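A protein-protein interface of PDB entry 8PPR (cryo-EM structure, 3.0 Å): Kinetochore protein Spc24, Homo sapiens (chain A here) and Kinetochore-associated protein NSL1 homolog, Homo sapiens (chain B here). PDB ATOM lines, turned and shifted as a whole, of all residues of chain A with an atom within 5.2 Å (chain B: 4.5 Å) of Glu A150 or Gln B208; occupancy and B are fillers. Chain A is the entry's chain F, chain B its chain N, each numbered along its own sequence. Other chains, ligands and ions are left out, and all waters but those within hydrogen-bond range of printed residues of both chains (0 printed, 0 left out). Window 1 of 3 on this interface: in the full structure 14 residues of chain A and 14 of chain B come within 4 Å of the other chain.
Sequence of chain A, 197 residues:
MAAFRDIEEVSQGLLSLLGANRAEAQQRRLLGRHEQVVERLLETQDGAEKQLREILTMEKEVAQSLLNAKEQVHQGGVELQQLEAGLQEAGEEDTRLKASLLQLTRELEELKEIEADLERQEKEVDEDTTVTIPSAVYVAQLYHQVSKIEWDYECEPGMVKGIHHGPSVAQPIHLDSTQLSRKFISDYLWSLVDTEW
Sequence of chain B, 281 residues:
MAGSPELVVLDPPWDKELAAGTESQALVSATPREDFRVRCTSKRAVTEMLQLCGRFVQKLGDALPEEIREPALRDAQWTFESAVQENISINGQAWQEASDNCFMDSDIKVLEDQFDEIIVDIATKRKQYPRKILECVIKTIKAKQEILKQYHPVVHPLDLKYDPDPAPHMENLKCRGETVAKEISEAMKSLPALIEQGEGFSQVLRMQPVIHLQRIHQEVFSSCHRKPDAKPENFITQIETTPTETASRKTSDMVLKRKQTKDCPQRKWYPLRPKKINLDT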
ATOM      1  N   HIS A 144     -20.272  -4.595  -8.083  1.00  0.00           N
ATOM      2  CA  HIS A 144     -19.735  -4.022  -6.854  1.00  0.00           C
ATOM      3  C   HIS A 144     -18.214  -4.080  -6.837  1.00  0.00           C
ATOM      4  O   HIS A 144     -17.555  -3.130  -6.403  1.00  0.00           O
ATOM      5  CB  HIS A 144     -20.320  -4.747  -5.645  1.00  0.00           C
ATOM      6  CG  HIS A 144     -19.633  -4.422  -4.359  1.00  0.00           C
ATOM      7  ND1 HIS A 144     -18.601  -5.180  -3.854  1.00  0.00           N
ATOM      8  CD2 HIS A 144     -19.824  -3.410  -3.480  1.00  0.00           C
ATOM      9  CE1 HIS A 144     -18.193  -4.655  -2.713  1.00  0.00           C
ATOM     10  NE2 HIS A 144     -18.916  -3.579  -2.465  1.00  0.00           N
ATOM     11  N   LYS A 148     -16.620  -0.896  -6.280  1.00  0.00           N
ATOM     12  CA  LYS A 148     -16.277  -0.787  -4.860  1.00  0.00           C
ATOM     13  C   LYS A 148     -17.250   0.142  -4.140  1.00  0.00           C
ATOM     14  O   LYS A 148     -16.872   0.909  -3.252  1.00  0.00           O
ATOM     15  CB  LYS A 148     -14.832  -0.325  -4.666  1.00  0.00           C
ATOM     16  CG  LYS A 148     -13.806  -1.238  -5.310  1.00  0.00           C
ATOM     17  CD  LYS A 148     -12.398  -0.719  -5.086  1.00  0.00           C
ATOM     18  CE  LYS A 148     -11.925  -1.019  -3.675  1.00  0.00           C
ATOM     19  NZ  LYS A 148     -11.754  -2.481  -3.450  1.00  0.00           N
ATOM     20  N   ILE A 149     -18.518   0.070  -4.535  1.00  0.00           N
ATOM     21  CA  ILE A 149     -19.567   0.940  -4.024  1.00  0.00           C
ATOM     22  C   ILE A 149     -20.677   0.085  -3.437  1.00  0.00           C
ATOM     23  O   ILE A 149     -21.176  -0.835  -4.092  1.00  0.00           O
ATOM     24  CB  ILE A 149     -20.122   1.860  -5.130  1.00  0.00           C
ATOM     25  CG1 ILE A 149     -19.026   2.796  -5.644  1.00  0.00           C
ATOM     26  CG2 ILE A 149     -21.342   2.618  -4.633  1.00  0.00           C
ATOM     27  CD1 ILE A 149     -19.511   3.815  -6.648  1.00  0.00           C
ATOM     28  N   GLU A 150     -21.071   0.402  -2.208  1.00  0.00           N
ATOM     29  CA  GLU A 150     -22.161  -0.281  -1.526  1.00  0.00           C
ATOM     30  C   GLU A 150     -23.303   0.706  -1.360  1.00  0.00           C
ATOM     31  O   GLU A 150     -23.120   1.773  -0.766  1.00  0.00           O
ATOM     32  CB  GLU A 150     -21.707  -0.816  -0.168  1.00  0.00           C
ATOM     33  CG  GLU A 150     -20.442  -1.650  -0.232  1.00  0.00           C
ATOM     34  CD  GLU A 150     -20.030  -2.184   1.121  1.00  0.00           C
ATOM     35  OE1 GLU A 150     -20.876  -2.196   2.040  1.00  0.00           O
ATOM     36  OE2 GLU A 150     -18.858  -2.586   1.270  1.00  0.00           O
ATOM     37  N   TRP A 151     -24.472   0.354  -1.879  1.00  0.00           N
ATOM     38  CA  TRP A 151     -25.611   1.256  -1.864  1.00  0.00           C
ATOM     39  C   TRP A 151     -26.400   1.132  -0.567  1.00  0.00           C
ATOM     40  O   TRP A 151     -26.380   0.104   0.112  1.00  0.00           O
ATOM     41  CB  TRP A 151     -26.533   0.987  -3.051  1.00  0.00           C
ATOM     42  CG  TRP A 151     -25.835   1.023  -4.362  1.00  0.00           C
ATOM     43  CD1 TRP A 151     -25.586  -0.030  -5.190  1.00  0.00           C
ATOM     44  CD2 TRP A 151     -25.292   2.178  -5.005  1.00  0.00           C
ATOM     45  NE1 TRP A 151     -24.920   0.399  -6.312  1.00  0.00           N
ATOM     46  CE2 TRP A 151     -24.727   1.751  -6.221  1.00  0.00           C
ATOM     47  CE3 TRP A 151     -25.229   3.533  -4.669  1.00  0.00           C
ATOM     48  CZ2 TRP A 151     -24.107   2.631  -7.103  1.00  0.00           C
ATOM     49  CZ3 TRP A 151     -24.613   4.403  -5.544  1.00  0.00           C
ATOM     50  CH2 TRP A 151     -24.058   3.949  -6.746  1.00  0.00           C
ATOM     51  N   ASP A 152     -27.106   2.207  -0.236  1.00  0.00           N
ATOM     52  CA  ASP A 152     -28.073   2.219   0.857  1.00  0.00           C
ATOM     53  C   ASP A 152     -29.447   2.038   0.222  1.00  0.00           C
ATOM     54  O   ASP A 152     -30.065   3.001  -0.236  1.00  0.00           O
ATOM     55  CB  ASP A 152     -27.981   3.512   1.658  1.00  0.00           C
ATOM     56  CG  ASP A 152     -28.618   3.396   3.028  1.00  0.00           C
ATOM     57  OD1 ASP A 152     -29.553   2.584   3.187  1.00  0.00           O
ATOM     58  OD2 ASP A 152     -28.180   4.115   3.951  1.00  0.00           O
ATOM     59  N   LYS A 161     -27.137   7.313  -2.058  1.00  0.00           N
ATOM     60  CA  LYS A 161     -26.512   7.148  -0.757  1.00  0.00           C
ATOM     61  C   LYS A 161     -25.738   5.841  -0.734  1.00  0.00           C
ATOM     62  O   LYS A 161     -26.210   4.822  -1.247  1.00  0.00           O
ATOM     63  CB  LYS A 161     -27.554   7.164   0.363  1.00  0.00           C
ATOM     64  CG  LYS A 161     -27.930   8.556   0.830  1.00  0.00           C
ATOM     65  CD  LYS A 161     -28.809   8.497   2.066  1.00  0.00           C
ATOM     66  CE  LYS A 161     -29.430   9.848   2.362  1.00  0.00           C
ATOM     67  NZ  LYS A 161     -30.329   9.793   3.547  1.00  0.00           N
ATOM     68  N   GLY A 162     -24.552   5.873  -0.137  1.00  0.00           N
ATOM     69  CA  GLY A 162     -23.755   4.667  -0.039  1.00  0.00           C
ATOM     70  C   GLY A 162     -22.338   4.973   0.399  1.00  0.00           C
ATOM     71  O   GLY A 162     -22.032   6.083   0.839  1.00  0.00           O
ATOM     72  N   ILE A 163     -21.482   3.966   0.261  1.00  0.00           N
ATOM     73  CA  ILE A 163     -20.095   4.024   0.703  1.00  0.00           C
ATOM     74  C   ILE A 163     -19.195   3.729  -0.486  1.00  0.00           C
ATOM     75  O   ILE A 163     -19.398   2.735  -1.193  1.00  0.00           O
ATOM     76  CB  ILE A 163     -19.823   3.028   1.845  1.00  0.00           C
ATOM     77  CG1 ILE A 163     -20.651   3.394   3.079  1.00  0.00           C
ATOM     78  CG2 ILE A 163     -18.338   2.971   2.158  1.00  0.00           C
ATOM     79  CD1 ILE A 163     -20.678   2.314   4.137  1.00  0.00           C
ATOM     80  N   HIS A 165     -15.464   2.751  -1.587  1.00  0.00           N
ATOM     81  CA  HIS A 165     -14.198   2.191  -1.146  1.00  0.00           C
ATOM     82  C   HIS A 165     -13.069   2.461  -2.131  1.00  0.00           C
ATOM     83  O   HIS A 165     -11.949   1.983  -1.923  1.00  0.00           O
ATOM     84  CB  HIS A 165     -14.345   0.688  -0.911  1.00  0.00           C
ATOM     85  CG  HIS A 165     -15.270   0.343   0.213  1.00  0.00           C
ATOM     86  ND1 HIS A 165     -14.824   0.090   1.493  1.00  0.00           N
ATOM     87  CD2 HIS A 165     -16.618   0.218   0.253  1.00  0.00           C
ATOM     88  CE1 HIS A 165     -15.857  -0.182   2.270  1.00  0.00           C
ATOM     89  NE2 HIS A 165     -16.956  -0.110   1.542  1.00  0.00           N
ATOM     90  N   VAL B 204     -18.977   6.854   7.485  1.00  0.00           N
ATOM     91  CA  VAL B 204     -18.982   5.559   6.810  1.00  0.00           C
ATOM     92  C   VAL B 204     -19.084   4.435   7.826  1.00  0.00           C
ATOM     93  O   VAL B 204     -19.860   3.486   7.656  1.00  0.00           O
ATOM     94  CB  VAL B 204     -17.716   5.404   5.948  1.00  0.00           C
ATOM     95  CG1 VAL B 204     -17.551   3.962   5.507  1.00  0.00           C
ATOM     96  CG2 VAL B 204     -17.785   6.306   4.757  1.00  0.00           C
ATOM     97  N   LEU B 205     -18.290   4.522   8.892  1.00  0.00           N
ATOM     98  CA  LEU B 205     -18.302   3.494   9.923  1.00  0.00           C
ATOM     99  C   LEU B 205     -19.669   3.384  10.576  1.00  0.00           C
ATOM    100  O   LEU B 205     -20.106   2.279  10.918  1.00  0.00           O
ATOM    101  CB  LEU B 205     -17.239   3.804  10.975  1.00  0.00           C
ATOM    102  CG  LEU B 205     -15.814   3.355  10.661  1.00  0.00           C
ATOM    103  CD1 LEU B 205     -14.861   3.797  11.760  1.00  0.00           C
ATOM    104  CD2 LEU B 205     -15.769   1.851  10.479  1.00  0.00           C
ATOM    105  N   ARG B 206     -20.354   4.510  10.760  1.00  0.00           N
ATOM    106  CA  ARG B 206     -21.650   4.471  11.420  1.00  0.00           C
ATOM    107  C   ARG B 206     -22.775   3.995  10.506  1.00  0.00           C
ATOM    108  O   ARG B 206     -23.762   3.454  11.013  1.00  0.00           O
ATOM    109  CB  ARG B 206     -21.991   5.836  12.020  1.00  0.00           C
ATOM    110  CG  ARG B 206     -22.358   6.904  11.025  1.00  0.00           C
ATOM    111  CD  ARG B 206     -23.048   8.059  11.710  1.00  0.00           C
ATOM    112  NE  ARG B 206     -22.278   8.506  12.863  1.00  0.00           N
ATOM    113  CZ  ARG B 206     -21.396   9.494  12.831  1.00  0.00           C
ATOM    114  NH1 ARG B 206     -21.154  10.169  11.719  1.00  0.00           N
ATOM    115  NH2 ARG B 206     -20.735   9.810  13.942  1.00  0.00           N
ATOM    116  N   MET B 207     -22.675   4.170   9.180  1.00  0.00           N
ATOM    117  CA  MET B 207     -23.668   3.508   8.328  1.00  0.00           C
ATOM    118  C   MET B 207     -23.269   2.115   7.861  1.00  0.00           C
ATOM    119  O   MET B 207     -24.075   1.460   7.193  1.00  0.00           O
ATOM    120  CB  MET B 207     -24.039   4.307   7.068  1.00  0.00           C
ATOM    121  CG  MET B 207     -24.979   5.477   7.266  1.00  0.00           C
ATOM    122  SD  MET B 207     -24.207   6.891   8.027  1.00  0.00           S
ATOM    123  CE  MET B 207     -23.281   7.419   6.588  1.00  0.00           C
ATOM    124  N   GLN B 208     -22.057   1.653   8.153  1.00  0.00           N
ATOM    125  CA  GLN B 208     -21.683   0.313   7.703  1.00  0.00           C
ATOM    126  C   GLN B 208     -22.598  -0.778   8.246  1.00  0.00           C
ATOM    127  O   GLN B 208     -23.058  -1.617   7.451  1.00  0.00           O
ATOM    128  CB  GLN B 208     -20.217   0.038   8.047  1.00  0.00           C
ATOM    129  CG  GLN B 208     -19.720  -1.288   7.503  1.00  0.00           C
ATOM    130  CD  GLN B 208     -19.624  -1.291   5.991  1.00  0.00           C
ATOM    131  OE1 GLN B 208     -20.487  -1.838   5.307  1.00  0.00           O
ATOM    132  NE2 GLN B 208     -18.579  -0.671   5.461  1.00  0.00           N
ATOM    133  N   PRO B 209     -22.911  -0.838   9.546  1.00  0.00           N
ATOM    134  CA  PRO B 209     -23.781  -1.931  10.010  1.00  0.00           C
ATOM    135  C   PRO B 209     -25.192  -1.851   9.460  1.00  0.00           C
ATOM    136  O   PRO B 209     -25.747  -2.880   9.055  1.00  0.00           O
ATOM    137  CB  PRO B 209     -23.754  -1.775  11.538  1.00  0.00           C
ATOM    138  CG  PRO B 209     -22.519  -0.982  11.819  1.00  0.00           C
ATOM    139  CD  PRO B 209     -22.425  -0.030  10.677  1.00  0.00           C
ATOM    140  N   VAL B 210     -25.790  -0.657   9.421  1.00  0.00           N
ATOM    141  CA  VAL B 210     -27.168  -0.543   8.955  1.00  0.00           C
ATOM    142  C   VAL B 210     -27.266  -0.894   7.477  1.00  0.00           C
ATOM    143  O   VAL B 210     -28.258  -1.489   7.037  1.00  0.00           O
ATOM    144  CB  VAL B 210     -27.730   0.864   9.254  1.00  0.00           C
ATOM    145  CG1 VAL B 210     -26.926   1.938   8.544  1.00  0.00           C
ATOM    146  CG2 VAL B 210     -29.200   0.944   8.868  1.00  0.00           C
ATOM    147  N   ILE B 211     -26.249  -0.542   6.690  1.00  0.00           N
ATOM    148  CA  ILE B 211     -26.213  -0.986   5.302  1.00  0.00           C
ATOM    149  C   ILE B 211     -26.063  -2.500   5.239  1.00  0.00           C
ATOM    150  O   ILE B 211     -26.716  -3.170   4.429  1.00  0.00           O
ATOM    151  CB  ILE B 211     -25.090  -0.265   4.535  1.00  0.00           C
ATOM    152  CG1 ILE B 211     -25.538   1.144   4.144  1.00  0.00           C
ATOM    153  CG2 ILE B 211     -24.688  -1.055   3.299  1.00  0.00           C
ATOM    154  CD1 ILE B 211     -24.488   1.931   3.392  1.00  0.00           C
ATOM    155  N   HIS B 212     -25.217  -3.066   6.103  1.00  0.00           N
ATOM    156  CA  HIS B 212     -25.062  -4.514   6.142  1.00  0.00           C
ATOM    157  C   HIS B 212     -26.336  -5.226   6.580  1.00  0.00           C
ATOM    158  O   HIS B 212     -26.497  -6.414   6.285  1.00  0.00           O
ATOM    159  CB  HIS B 212     -23.911  -4.894   7.071  1.00  0.00           C
ATOM    160  CG  HIS B 212     -22.583  -4.955   6.385  1.00  0.00           C
ATOM    161  ND1 HIS B 212     -21.565  -5.785   6.804  1.00  0.00           N
ATOM    162  CD2 HIS B 212     -22.113  -4.301   5.298  1.00  0.00           C
ATOM    163  CE1 HIS B 212     -20.521  -5.630   6.010  1.00  0.00           C
ATOM    164  NE2 HIS B 212     -20.826  -4.735   5.089  1.00  0.00           N
ATOM    165  N   HIS B 217     -28.893  -5.974   0.363  1.00  0.00           N
ATOM    166  CA  HIS B 217     -27.454  -6.130   0.532  1.00  0.00           C
ATOM    167  C   HIS B 217     -27.107  -7.537   0.999  1.00  0.00           C
ATOM    168  O   HIS B 217     -26.139  -8.138   0.519  1.00  0.00           O
ATOM    169  CB  HIS B 217     -26.937  -5.089   1.525  1.00  0.00           C
ATOM    170  CG  HIS B 217     -25.490  -5.246   1.871  1.00  0.00           C
ATOM    171  ND1 HIS B 217     -25.037  -6.186   2.772  1.00  0.00           N
ATOM    172  CD2 HIS B 217     -24.394  -4.575   1.445  1.00  0.00           C
ATOM    173  CE1 HIS B 217     -23.725  -6.093   2.881  1.00  0.00           C
ATOM    174  NE2 HIS B 217     -23.308  -5.123   2.086  1.00  0.00           N
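OE1 of Glu A150 sits close to OE1 of Gln B208 (3.3 Å).
OE1 of Gln B208 sits at hydrogen-bond distance from NE2 of His B212, 2.9 Å away. The backbone NH (N) of Ile A163 sits at hydrogen-bond distance from the backbone carbonyl oxygen (O) of Glu A150, 2.9 Å away. OE2 of Glu A150 sits at hydrogen-bond distance from NE2 of His A165, 3.1 Å away. The backbone NH (N) of Asp A152 lies within hydrogen-bond range of the backbone carbonyl oxygen (O) of Lys A161 (2.9 Å).
OE1 of Glu A150 touches NE2 of His B212, 3.97 Å away. Glu A150 touches His B217 (OE1 to NE2, 3.8 Å). O of Trp A151 touches CG2 of Ile B211, 3.8 Å away. CG1 of Ile B211 touches CG of Asp A152, 3.98 Å away. CG2 of Ile A163 touches CG1 of Val B204, 3.6 Å away. Ile A163 touches Gln B208 (CD1 to NE2, 3.9 Å). Ile A163 touches Ile B211 (CD1 to CD1, 3.9 Å).
Glu A150 touches three residues of chain B. Of chain A, only Glu A150 (3.3 Å) and Ile A163 (3.9 Å) come within 4 Å of Gln B208. Printed residues of chain B within 4 Å of Trp A151: Ile B211 (3.8 Å). Of the printed residues of chain A, Ile B211 touches Trp A151 (3.8 Å), Asp A152 (3.98 Å) and Ile A163 (3.9 Å). Of the printed residues of chain A, His B212 touches Glu A150 (3.97 Å). Printed residues of chain B within 4 Å of Ile A163: Val B204 (3.6 Å), Gln B208 (3.9 Å) and Ile B211 (3.9 Å). Of the printed residues of chain B, Asp A152 touches Ile B211. The nearest residue of chain B that does not touch Glu A150 is Ile B211 (4.2 Å).
Hydrophobic or aromatic side chains of chain A that line the printed part of chain B: Ile A163.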
